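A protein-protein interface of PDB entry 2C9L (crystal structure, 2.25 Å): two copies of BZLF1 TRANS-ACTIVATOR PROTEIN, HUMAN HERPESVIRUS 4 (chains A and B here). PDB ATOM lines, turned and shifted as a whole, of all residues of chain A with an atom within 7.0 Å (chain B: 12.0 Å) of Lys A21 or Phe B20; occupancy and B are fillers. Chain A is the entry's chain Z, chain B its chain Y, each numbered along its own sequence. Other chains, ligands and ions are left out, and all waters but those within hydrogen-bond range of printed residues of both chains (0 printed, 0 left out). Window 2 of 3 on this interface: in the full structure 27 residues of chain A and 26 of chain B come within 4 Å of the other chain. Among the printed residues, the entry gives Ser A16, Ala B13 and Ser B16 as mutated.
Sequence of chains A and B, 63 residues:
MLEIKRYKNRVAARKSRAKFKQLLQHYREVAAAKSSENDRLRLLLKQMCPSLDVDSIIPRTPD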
ATOM      1  N   LYS A  15      11.111  30.360 -42.729  1.00  0.00           N
ATOM      2  CA  LYS A  15      12.540  30.122 -42.567  1.00  0.00           C
ATOM      3  C   LYS A  15      13.030  30.551 -41.183  1.00  0.00           C
ATOM      4  O   LYS A  15      13.735  29.802 -40.503  1.00  0.00           O
ATOM      5  CB  LYS A  15      13.316  30.860 -43.664  1.00  0.00           C
ATOM      6  CG  LYS A  15      14.830  30.665 -43.603  1.00  0.00           C
ATOM      7  CD  LYS A  15      15.519  31.377 -44.761  1.00  0.00           C
ATOM      8  CE  LYS A  15      17.031  31.279 -44.653  1.00  0.00           C
ATOM      9  NZ  LYS A  15      17.709  31.975 -45.786  1.00  0.00           N
ATOM     10  N   SER A  16      12.643  31.754 -40.763  1.00  0.00           N
ATOM     11  CA  SER A  16      13.045  32.265 -39.456  1.00  0.00           C
ATOM     12  C   SER A  16      12.564  31.322 -38.348  1.00  0.00           C
ATOM     13  O   SER A  16      13.317  31.002 -37.434  1.00  0.00           O
ATOM     14  CB  SER A  16      12.485  33.679 -39.250  1.00  0.00           C
ATOM     15  OG  SER A  16      12.980  34.258 -38.054  1.00  0.00           O
ATOM     16  N   ARG A  17      11.322  30.855 -38.445  1.00  0.00           N
ATOM     17  CA  ARG A  17      10.776  29.928 -37.448  1.00  0.00           C
ATOM     18  C   ARG A  17      11.436  28.544 -37.465  1.00  0.00           C
ATOM     19  O   ARG A  17      11.520  27.873 -36.429  1.00  0.00           O
ATOM     20  CB  ARG A  17       9.265  29.778 -37.641  1.00  0.00           C
ATOM     21  CG  ARG A  17       8.489  30.988 -37.140  1.00  0.00           C
ATOM     22  CD  ARG A  17       7.023  30.992 -37.571  1.00  0.00           C
ATOM     23  NE  ARG A  17       6.355  32.163 -37.006  1.00  0.00           N
ATOM     24  CZ  ARG A  17       5.428  32.891 -37.623  1.00  0.00           C
ATOM     25  NH1 ARG A  17       5.029  32.593 -38.847  1.00  0.00           N
ATOM     26  NH2 ARG A  17       4.896  33.932 -37.001  1.00  0.00           N
ATOM     27  N   ALA A  18      11.896  28.104 -38.631  1.00  0.00           N
ATOM     28  CA  ALA A  18      12.554  26.796 -38.712  1.00  0.00           C
ATOM     29  C   ALA A  18      13.938  26.913 -38.076  1.00  0.00           C
ATOM     30  O   ALA A  18      14.362  26.045 -37.308  1.00  0.00           O
ATOM     31  CB  ALA A  18      12.674  26.345 -40.169  1.00  0.00           C
ATOM     32  N   LYS A  19      14.627  28.003 -38.382  1.00  0.00           N
ATOM     33  CA  LYS A  19      15.958  28.237 -37.828  1.00  0.00           C
ATOM     34  C   LYS A  19      15.924  28.104 -36.310  1.00  0.00           C
ATOM     35  O   LYS A  19      16.734  27.387 -35.720  1.00  0.00           O
ATOM     36  CB  LYS A  19      16.487  29.605 -38.201  1.00  0.00           C
ATOM     37  CG  LYS A  19      17.717  30.018 -37.405  1.00  0.00           C
ATOM     38  CD  LYS A  19      18.107  31.471 -37.663  1.00  0.00           C
ATOM     39  CE  LYS A  19      19.181  31.918 -36.684  1.00  0.00           C
ATOM     40  NZ  LYS A  19      19.552  33.344 -36.862  1.00  0.00           N
ATOM     41  N   PHE A  20      14.967  28.790 -35.693  1.00  0.00           N
ATOM     42  CA  PHE A  20      14.803  28.765 -34.248  1.00  0.00           C
ATOM     43  C   PHE A  20      14.400  27.380 -33.765  1.00  0.00           C
ATOM     44  O   PHE A  20      14.987  26.849 -32.823  1.00  0.00           O
ATOM     45  CB  PHE A  20      13.730  29.771 -33.826  1.00  0.00           C
ATOM     46  CG  PHE A  20      13.426  29.748 -32.356  1.00  0.00           C
ATOM     47  CD1 PHE A  20      14.272  30.369 -31.445  1.00  0.00           C
ATOM     48  CD2 PHE A  20      12.294  29.096 -31.879  1.00  0.00           C
ATOM     49  CE1 PHE A  20      13.996  30.341 -30.078  1.00  0.00           C
ATOM     50  CE2 PHE A  20      12.009  29.060 -30.514  1.00  0.00           C
ATOM     51  CZ  PHE A  20      12.862  29.686 -29.613  1.00  0.00           C
ATOM     52  N   LYS A  21      13.388  26.804 -34.410  1.00  0.00           N
ATOM     53  CA  LYS A  21      12.896  25.486 -34.032  1.00  0.00           C
ATOM     54  C   LYS A  21      14.042  24.473 -34.152  1.00  0.00           C
ATOM     55  O   LYS A  21      14.199  23.598 -33.304  1.00  0.00           O
ATOM     56  CB  LYS A  21      11.738  25.055 -34.942  1.00  0.00           C
ATOM     57  CG  LYS A  21      10.409  25.759 -34.685  1.00  0.00           C
ATOM     58  CD  LYS A  21       9.920  25.487 -33.276  1.00  0.00           C
ATOM     59  CE  LYS A  21       8.531  26.072 -33.045  1.00  0.00           C
ATOM     60  NZ  LYS A  21       8.050  25.780 -31.665  1.00  0.00           N
ATOM     61  N   GLN A  22      14.841  24.604 -35.208  1.00  0.00           N
ATOM     62  CA  GLN A  22      15.970  23.700 -35.423  1.00  0.00           C
ATOM     63  C   GLN A  22      17.012  23.866 -34.319  1.00  0.00           C
ATOM     64  O   GLN A  22      17.485  22.881 -33.759  1.00  0.00           O
ATOM     65  CB  GLN A  22      16.615  23.962 -36.793  1.00  0.00           C
ATOM     66  CG  GLN A  22      15.722  23.598 -37.973  1.00  0.00           C
ATOM     67  CD  GLN A  22      16.474  23.571 -39.291  1.00  0.00           C
ATOM     68  OE1 GLN A  22      17.385  22.763 -39.479  1.00  0.00           O
ATOM     69  NE2 GLN A  22      16.097  24.457 -40.212  1.00  0.00           N
ATOM     70  N   LEU A  23      17.358  25.113 -34.007  1.00  0.00           N
ATOM     71  CA  LEU A  23      18.327  25.389 -32.951  1.00  0.00           C
ATOM     72  C   LEU A  23      17.893  24.723 -31.662  1.00  0.00           C
ATOM     73  O   LEU A  23      18.673  24.030 -31.016  1.00  0.00           O
ATOM     74  CB  LEU A  23      18.459  26.895 -32.710  1.00  0.00           C
ATOM     75  CG  LEU A  23      19.535  27.639 -33.500  1.00  0.00           C
ATOM     76  CD1 LEU A  23      19.500  29.124 -33.140  1.00  0.00           C
ATOM     77  CD2 LEU A  23      20.903  27.042 -33.181  1.00  0.00           C
ATOM     78  N   LEU A  24      16.630  24.923 -31.308  1.00  0.00           N
ATOM     79  CA  LEU A  24      16.070  24.358 -30.091  1.00  0.00           C
ATOM     80  C   LEU A  24      16.144  22.845 -30.079  1.00  0.00           C
ATOM     81  O   LEU A  24      16.524  22.246 -29.077  1.00  0.00           O
ATOM     82  CB  LEU A  24      14.616  24.801 -29.916  1.00  0.00           C
ATOM     83  CG  LEU A  24      13.861  24.054 -28.814  1.00  0.00           C
ATOM     84  CD1 LEU A  24      14.550  24.265 -27.475  1.00  0.00           C
ATOM     85  CD2 LEU A  24      12.420  24.540 -28.764  1.00  0.00           C
ATOM     86  N   GLN A  25      15.767  22.227 -31.194  1.00  0.00           N
ATOM     87  CA  GLN A  25      15.810  20.777 -31.302  1.00  0.00           C
ATOM     88  C   GLN A  25      17.267  20.334 -31.190  1.00  0.00           C
ATOM     89  O   GLN A  25      17.577  19.371 -30.504  1.00  0.00           O
ATOM     90  CB  GLN A  25      15.220  20.333 -32.645  1.00  0.00           C
ATOM     91  CG  GLN A  25      15.097  18.822 -32.830  1.00  0.00           C
ATOM     92  CD  GLN A  25      14.488  18.460 -34.178  1.00  0.00           C
ATOM     93  OE1 GLN A  25      14.966  18.904 -35.220  1.00  0.00           O
ATOM     94  NE2 GLN A  25      13.433  17.652 -34.161  1.00  0.00           N
ATOM     95  N   HIS A  26      18.159  21.055 -31.856  1.00  0.00           N
ATOM     96  CA  HIS A  26      19.592  20.738 -31.818  1.00  0.00           C
ATOM     97  C   HIS A  26      20.164  20.707 -30.393  1.00  0.00           C
ATOM     98  O   HIS A  26      20.777  19.715 -29.980  1.00  0.00           O
ATOM     99  CB  HIS A  26      20.362  21.754 -32.661  1.00  0.00           C
ATOM    100  CG  HIS A  26      21.849  21.607 -32.583  1.00  0.00           C
ATOM    101  ND1 HIS A  26      22.517  20.512 -33.087  1.00  0.00           N
ATOM    102  CD2 HIS A  26      22.800  22.423 -32.069  1.00  0.00           C
ATOM    103  CE1 HIS A  26      23.814  20.658 -32.887  1.00  0.00           C
ATOM    104  NE2 HIS A  26      24.013  21.810 -32.271  1.00  0.00           N
ATOM    105  N   VAL B  11      -2.293  38.070 -25.089  1.00  0.00           N
ATOM    106  CA  VAL B  11      -1.499  37.832 -23.884  1.00  0.00           C
ATOM    107  C   VAL B  11      -0.844  36.443 -23.954  1.00  0.00           C
ATOM    108  O   VAL B  11       0.330  36.291 -23.632  1.00  0.00           O
ATOM    109  CB  VAL B  11      -2.368  37.922 -22.610  1.00  0.00           C
ATOM    110  CG1 VAL B  11      -1.576  37.453 -21.378  1.00  0.00           C
ATOM    111  CG2 VAL B  11      -2.833  39.366 -22.411  1.00  0.00           C
ATOM    112  N   ALA B  12      -1.609  35.441 -24.378  1.00  0.00           N
ATOM    113  CA  ALA B  12      -1.095  34.074 -24.493  1.00  0.00           C
ATOM    114  C   ALA B  12      -0.002  33.930 -25.551  1.00  0.00           C
ATOM    115  O   ALA B  12       0.928  33.153 -25.358  1.00  0.00           O
ATOM    116  CB  ALA B  12      -2.228  33.105 -24.772  1.00  0.00           C
ATOM    117  N   ALA B  13      -0.097  34.668 -26.660  1.00  0.00           N
ATOM    118  CA  ALA B  13       0.944  34.592 -27.688  1.00  0.00           C
ATOM    119  C   ALA B  13       2.234  35.174 -27.124  1.00  0.00           C
ATOM    120  O   ALA B  13       3.307  34.610 -27.334  1.00  0.00           O
ATOM    121  CB  ALA B  13       0.546  35.345 -28.947  1.00  0.00           C
ATOM    122  N   ARG B  14       2.139  36.310 -26.425  1.00  0.00           N
ATOM    123  CA  ARG B  14       3.329  36.915 -25.821  1.00  0.00           C
ATOM    124  C   ARG B  14       3.974  35.905 -24.870  1.00  0.00           C
ATOM    125  O   ARG B  14       5.187  35.726 -24.869  1.00  0.00           O
ATOM    126  CB  ARG B  14       2.975  38.176 -25.019  1.00  0.00           C
ATOM    127  CG  ARG B  14       2.609  39.379 -25.862  1.00  0.00           C
ATOM    128  CD  ARG B  14       1.950  40.488 -25.037  1.00  0.00           C
ATOM    129  NE  ARG B  14       1.462  41.535 -25.928  1.00  0.00           N
ATOM    130  CZ  ARG B  14       0.622  42.506 -25.583  1.00  0.00           C
ATOM    131  NH1 ARG B  14       0.154  42.588 -24.341  1.00  0.00           N
ATOM    132  NH2 ARG B  14       0.239  43.387 -26.494  1.00  0.00           N
ATOM    133  N   LYS B  15       3.150  35.252 -24.060  1.00  0.00           N
ATOM    134  CA  LYS B  15       3.660  34.279 -23.102  1.00  0.00           C
ATOM    135  C   LYS B  15       4.301  33.069 -23.778  1.00  0.00           C
ATOM    136  O   LYS B  15       5.331  32.566 -23.320  1.00  0.00           O
ATOM    137  CB  LYS B  15       2.541  33.797 -22.191  1.00  0.00           C
ATOM    138  CG  LYS B  15       2.986  32.744 -21.173  1.00  0.00           C
ATOM    139  CD  LYS B  15       1.815  32.255 -20.320  1.00  0.00           C
ATOM    140  CE  LYS B  15       2.262  31.202 -19.298  1.00  0.00           C
ATOM    141  NZ  LYS B  15       1.095  30.537 -18.634  1.00  0.00           N
ATOM    142  N   SER B  16       3.683  32.613 -24.866  1.00  0.00           N
ATOM    143  CA  SER B  16       4.168  31.459 -25.599  1.00  0.00           C
ATOM    144  C   SER B  16       5.499  31.766 -26.242  1.00  0.00           C
ATOM    145  O   SER B  16       6.426  30.968 -26.169  1.00  0.00           O
ATOM    146  CB  SER B  16       3.161  31.043 -26.673  1.00  0.00           C
ATOM    147  OG  SER B  16       3.560  29.837 -27.282  1.00  0.00           O
ATOM    148  N   ARG B  17       5.596  32.935 -26.864  1.00  0.00           N
ATOM    149  CA  ARG B  17       6.835  33.343 -27.506  1.00  0.00           C
ATOM    150  C   ARG B  17       7.974  33.488 -26.499  1.00  0.00           C
ATOM    151  O   ARG B  17       9.106  33.091 -26.777  1.00  0.00           O
ATOM    152  CB  ARG B  17       6.637  34.662 -28.258  1.00  0.00           C
ATOM    153  CG  ARG B  17       6.168  34.482 -29.692  1.00  0.00           C
ATOM    154  CD  ARG B  17       5.897  35.813 -30.363  1.00  0.00           C
ATOM    155  NE  ARG B  17       4.598  36.357 -29.984  1.00  0.00           N
ATOM    156  CZ  ARG B  17       4.420  37.490 -29.314  1.00  0.00           C
ATOM    157  NH1 ARG B  17       5.460  38.221 -28.934  1.00  0.00           N
ATOM    158  NH2 ARG B  17       3.192  37.899 -29.036  1.00  0.00           N
ATOM    159  N   ALA B  18       7.677  34.049 -25.329  1.00  0.00           N
ATOM    160  CA  ALA B  18       8.709  34.234 -24.302  1.00  0.00           C
ATOM    161  C   ALA B  18       9.070  32.864 -23.754  1.00  0.00           C
ATOM    162  O   ALA B  18      10.225  32.602 -23.447  1.00  0.00           O
ATOM    163  CB  ALA B  18       8.212  35.148 -23.157  1.00  0.00           C
ATOM    164  N   LYS B  19       8.071  31.992 -23.644  1.00  0.00           N
ATOM    165  CA  LYS B  19       8.297  30.638 -23.162  1.00  0.00           C
ATOM    166  C   LYS B  19       9.256  29.880 -24.086  1.00  0.00           C
ATOM    167  O   LYS B  19      10.093  29.108 -23.623  1.00  0.00           O
ATOM    168  CB  LYS B  19       6.989  29.863 -23.078  1.00  0.00           C
ATOM    169  CG  LYS B  19       7.190  28.406 -22.677  1.00  0.00           C
ATOM    170  CD  LYS B  19       5.918  27.588 -22.843  1.00  0.00           C
ATOM    171  CE  LYS B  19       6.219  26.090 -22.766  1.00  0.00           C
ATOM    172  NZ  LYS B  19       5.020  25.240 -23.030  1.00  0.00           N
ATOM    173  N   PHE B  20       9.133  30.088 -25.392  1.00  0.00           N
ATOM    174  CA  PHE B  20      10.015  29.400 -26.328  1.00  0.00           C
ATOM    175  C   PHE B  20      11.426  29.977 -26.307  1.00  0.00           C
ATOM    176  O   PHE B  20      12.399  29.236 -26.413  1.00  0.00           O
ATOM    177  CB  PHE B  20       9.435  29.434 -27.746  1.00  0.00           C
ATOM    178  CG  PHE B  20       8.438  28.340 -28.009  1.00  0.00           C
ATOM    179  CD1 PHE B  20       8.823  27.003 -27.937  1.00  0.00           C
ATOM    180  CD2 PHE B  20       7.114  28.638 -28.311  1.00  0.00           C
ATOM    181  CE1 PHE B  20       7.906  25.980 -28.162  1.00  0.00           C
ATOM    182  CE2 PHE B  20       6.189  27.623 -28.537  1.00  0.00           C
ATOM    183  CZ  PHE B  20       6.586  26.290 -28.461  1.00  0.00           C
ATOM    184  N   LYS B  21      11.539  31.296 -26.169  1.00  0.00           N
ATOM    185  CA  LYS B  21      12.851  31.931 -26.097  1.00  0.00           C
ATOM    186  C   LYS B  21      13.623  31.468 -24.855  1.00  0.00           C
ATOM    187  O   LYS B  21      14.828  31.235 -24.922  1.00  0.00           O
ATOM    188  CB  LYS B  21      12.712  33.455 -26.074  1.00  0.00           C
ATOM    189  CG  LYS B  21      12.318  34.064 -27.408  1.00  0.00           C
ATOM    190  CD  LYS B  21      13.395  33.840 -28.457  1.00  0.00           C
ATOM    191  CE  LYS B  21      13.027  34.491 -29.784  1.00  0.00           C
ATOM    192  NZ  LYS B  21      14.103  34.340 -30.809  1.00  0.00           N
ATOM    193  N   GLN B  22      12.932  31.332 -23.727  1.00  0.00           N
ATOM    194  CA  GLN B  22      13.586  30.891 -22.499  1.00  0.00           C
ATOM    195  C   GLN B  22      13.959  29.414 -22.590  1.00  0.00           C
ATOM    196  O   GLN B  22      14.974  28.984 -22.050  1.00  0.00           O
ATOM    197  CB  GLN B  22      12.675  31.128 -21.292  1.00  0.00           C
ATOM    198  CG  GLN B  22      11.345  30.389 -21.330  1.00  0.00           C
ATOM    199  CD  GLN B  22      11.423  28.989 -20.750  1.00  0.00           C
ATOM    200  OE1 GLN B  22      10.428  28.254 -20.732  1.00  0.00           O
ATOM    201  NE2 GLN B  22      12.602  28.613 -20.262  1.00  0.00           N
ATOM    202  N   LEU B  23      13.138  28.646 -23.295  1.00  0.00           N
ATOM    203  CA  LEU B  23      13.385  27.225 -23.455  1.00  0.00           C
ATOM    204  C   LEU B  23      14.683  27.032 -24.230  1.00  0.00           C
ATOM    205  O   LEU B  23      15.501  26.185 -23.881  1.00  0.00           O
ATOM    206  CB  LEU B  23      12.210  26.581 -24.183  1.00  0.00           C
ATOM    207  CG  LEU B  23      11.913  25.104 -23.918  1.00  0.00           C
ATOM    208  CD1 LEU B  23      11.831  24.838 -22.417  1.00  0.00           C
ATOM    209  CD2 LEU B  23      10.592  24.744 -24.604  1.00  0.00           C
ATOM    210  N   LEU B  24      14.874  27.844 -25.266  1.00  0.00           N
ATOM    211  CA  LEU B  24      16.078  27.790 -26.085  1.00  0.00           C
ATOM    212  C   LEU B  24      17.315  28.210 -25.289  1.00  0.00           C
ATOM    213  O   LEU B  24      18.406  27.659 -25.470  1.00  0.00           O
ATOM    214  CB  LEU B  24      15.954  28.717 -27.292  1.00  0.00           C
ATOM    215  CG  LEU B  24      17.235  28.772 -28.127  1.00  0.00           C
ATOM    216  CD1 LEU B  24      17.380  27.470 -28.904  1.00  0.00           C
ATOM    217  CD2 LEU B  24      17.197  29.961 -29.074  1.00  0.00           C
ATOM    218  N   GLN B  25      17.141  29.206 -24.429  1.00  0.00           N
ATOM    219  CA  GLN B  25      18.232  29.717 -23.606  1.00  0.00           C
ATOM    220  C   GLN B  25      18.624  28.634 -22.604  1.00  0.00           C
ATOM    221  O   GLN B  25      19.800  28.410 -22.343  1.00  0.00           O
ATOM    222  CB  GLN B  25      17.768  30.984 -22.876  1.00  0.00           C
ATOM    223  CG  GLN B  25      18.873  31.908 -22.372  1.00  0.00           C
ATOM    224  CD  GLN B  25      19.570  31.393 -21.132  1.00  0.00           C
ATOM    225  OE1 GLN B  25      18.926  31.048 -20.140  1.00  0.00           O
ATOM    226  NE2 GLN B  25      20.899  31.353 -21.175  1.00  0.00           N
ATOM    227  N   HIS B  26      17.617  27.955 -22.072  1.00  0.00           N
ATOM    228  CA  HIS B  26      17.799  26.892 -21.093  1.00  0.00           C
ATOM    229  C   HIS B  26      18.563  25.675 -21.630  1.00  0.00           C
ATOM    230  O   HIS B  26      19.510  25.192 -21.000  1.00  0.00           O
ATOM    231  CB  HIS B  26      16.429  26.449 -20.578  1.00  0.00           C
ATOM    232  CG  HIS B  26      16.481  25.283 -19.643  1.00  0.00           C
ATOM    233  ND1 HIS B  26      16.837  25.405 -18.316  1.00  0.00           N
ATOM    234  CD2 HIS B  26      16.225  23.969 -19.844  1.00  0.00           C
ATOM    235  CE1 HIS B  26      16.795  24.215 -17.741  1.00  0.00           C
ATOM    236  NE2 HIS B  26      16.427  23.327 -18.647  1.00  0.00           N
ATOM    237  N   TYR B  27      18.153  25.169 -22.786  1.00  0.00           N
ATOM    238  CA  TYR B  27      18.823  23.997 -23.356  1.00  0.00           C
ATOM    239  C   TYR B  27      20.209  24.309 -23.888  1.00  0.00           C
ATOM    240  O   TYR B  27      21.054  23.422 -24.020  1.00  0.00           O
ATOM    241  CB  TYR B  27      17.950  23.367 -24.447  1.00  0.00           C
ATOM    242  CG  TYR B  27      16.823  22.540 -23.863  1.00  0.00           C
ATOM    243  CD1 TYR B  27      17.098  21.469 -23.013  1.00  0.00           C
ATOM    244  CD2 TYR B  27      15.489  22.856 -24.113  1.00  0.00           C
ATOM    245  CE1 TYR B  27      16.076  20.735 -22.419  1.00  0.00           C
ATOM    246  CE2 TYR B  27      14.455  22.125 -23.521  1.00  0.00           C
ATOM    247  CZ  TYR B  27      14.760  21.067 -22.673  1.00  0.00           C
ATOM    248  OH  TYR B  27      13.756  20.346 -22.068  1.00  0.00           O
ATOM    249  N   ARG B  28      20.448  25.580 -24.183  1.00  0.00           N
ATOM    250  CA  ARG B  28      21.747  26.007 -24.675  1.00  0.00           C
ATOM    251  C   ARG B  28      22.729  25.909 -23.489  1.00  0.00           C
ATOM    252  O   ARG B  28      23.871  25.472 -23.646  1.00  0.00           O
ATOM    253  CB  ARG B  28      21.639  27.445 -25.160  1.00  0.00           C
ATOM    254  CG  ARG B  28      22.700  27.923 -26.121  1.00  0.00           C
ATOM    255  CD  ARG B  28      22.462  29.403 -26.420  1.00  0.00           C
ATOM    256  NE  ARG B  28      22.717  29.758 -27.814  1.00  0.00           N
ATOM    257  CZ  ARG B  28      23.920  29.789 -28.380  1.00  0.00           C
ATOM    258  NH1 ARG B  28      24.999  29.486 -27.670  1.00  0.00           N
ATOM    259  NH2 ARG B  28      24.042  30.121 -29.659  1.00  0.00           N
ATOM    260  N   GLU B  29      22.258  26.299 -22.305  1.00  0.00           N
ATOM    261  CA  GLU B  29      23.063  26.281 -21.079  1.00  0.00           C
ATOM    262  C   GLU B  29      23.300  24.868 -20.556  1.00  0.00           C
ATOM    263  O   GLU B  29      24.399  24.541 -20.124  1.00  0.00           O
ATOM    264  CB  GLU B  29      22.380  27.089 -19.970  1.00  0.00           C
ATOM    265  CG  GLU B  29      22.135  28.544 -20.293  1.00  0.00           C
ATOM    266  CD  GLU B  29      21.498  29.290 -19.132  1.00  0.00           C
ATOM    267  OE1 GLU B  29      20.493  28.789 -18.580  1.00  0.00           O
ATOM    268  OE2 GLU B  29      21.997  30.380 -18.777  1.00  0.00           O
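Hydrophobic or aromatic side chains of chain A within 4 Å of the printed part of chain B: Phe A20, Leu A23 and Leu A24.
Hydrophobic or aromatic side chains of chain B that line the printed part of chain A: Phe B20, Leu B24 and Tyr B27.
Among the printed residues, no Asp or Glu carboxylate lies within 4 Å of a Lys or Arg side-chain nitrogen of the other chain.
Arg A17 touches none of the printed residues of chain B.
No residue of chain B comes within 4 Å of Gln A22.
Of the printed residues of chain B, Leu A23 touches Leu B24 (3.9 Å).
Printed residues of chain B within 4 Å of Leu A24: Leu B24 and Tyr B27.
Gln A25 touches none of the printed residues of chain B.
Val B11 touches none of the printed residues of chain A.
Printed residues of chain A within 4 Å of Phe B20: Phe A20 (3.3 Å) and Lys A21 (3.5 Å).
Of the printed residues of chain A, Tyr B27 touches Leu A24 (3.8 Å).
The nearest printed residue of chain B that does not touch Lys A21 is Leu B24 (6.7 Å).
The nearest printed residue of chain B that does not touch Leu A24 is Leu B23 (4.2 Å).
O of Phe B20 touches CZ of Phe A20 (3.3 Å).
Lys B21 touches Phe A20 (CD to CE1, 3.9 Å).
Phe A20 touches Leu B24.
NZ of Lys A21 touches CE1 of Phe B20 (3.5 Å).
C of Leu A23 touches CD1 of Leu B24, at 3.9 Å.
CD1 of Leu B24 touches CA of Leu A24, 3.6 Å away.
Leu A24 touches Tyr B27.
Phe B20 touches its own counterpart, Phe A20.
Phe A20 touches Leu B24, but with the chains exchanged Leu A24 does not touch Phe B20 (4.4 Å).
Leu A23 touches Leu B24, but with the chains exchanged Leu A24 does not touch Leu B23 (4.2 Å).
Leu B24 touches its own counterpart, Leu A24.
12 positions are printed for both chains.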
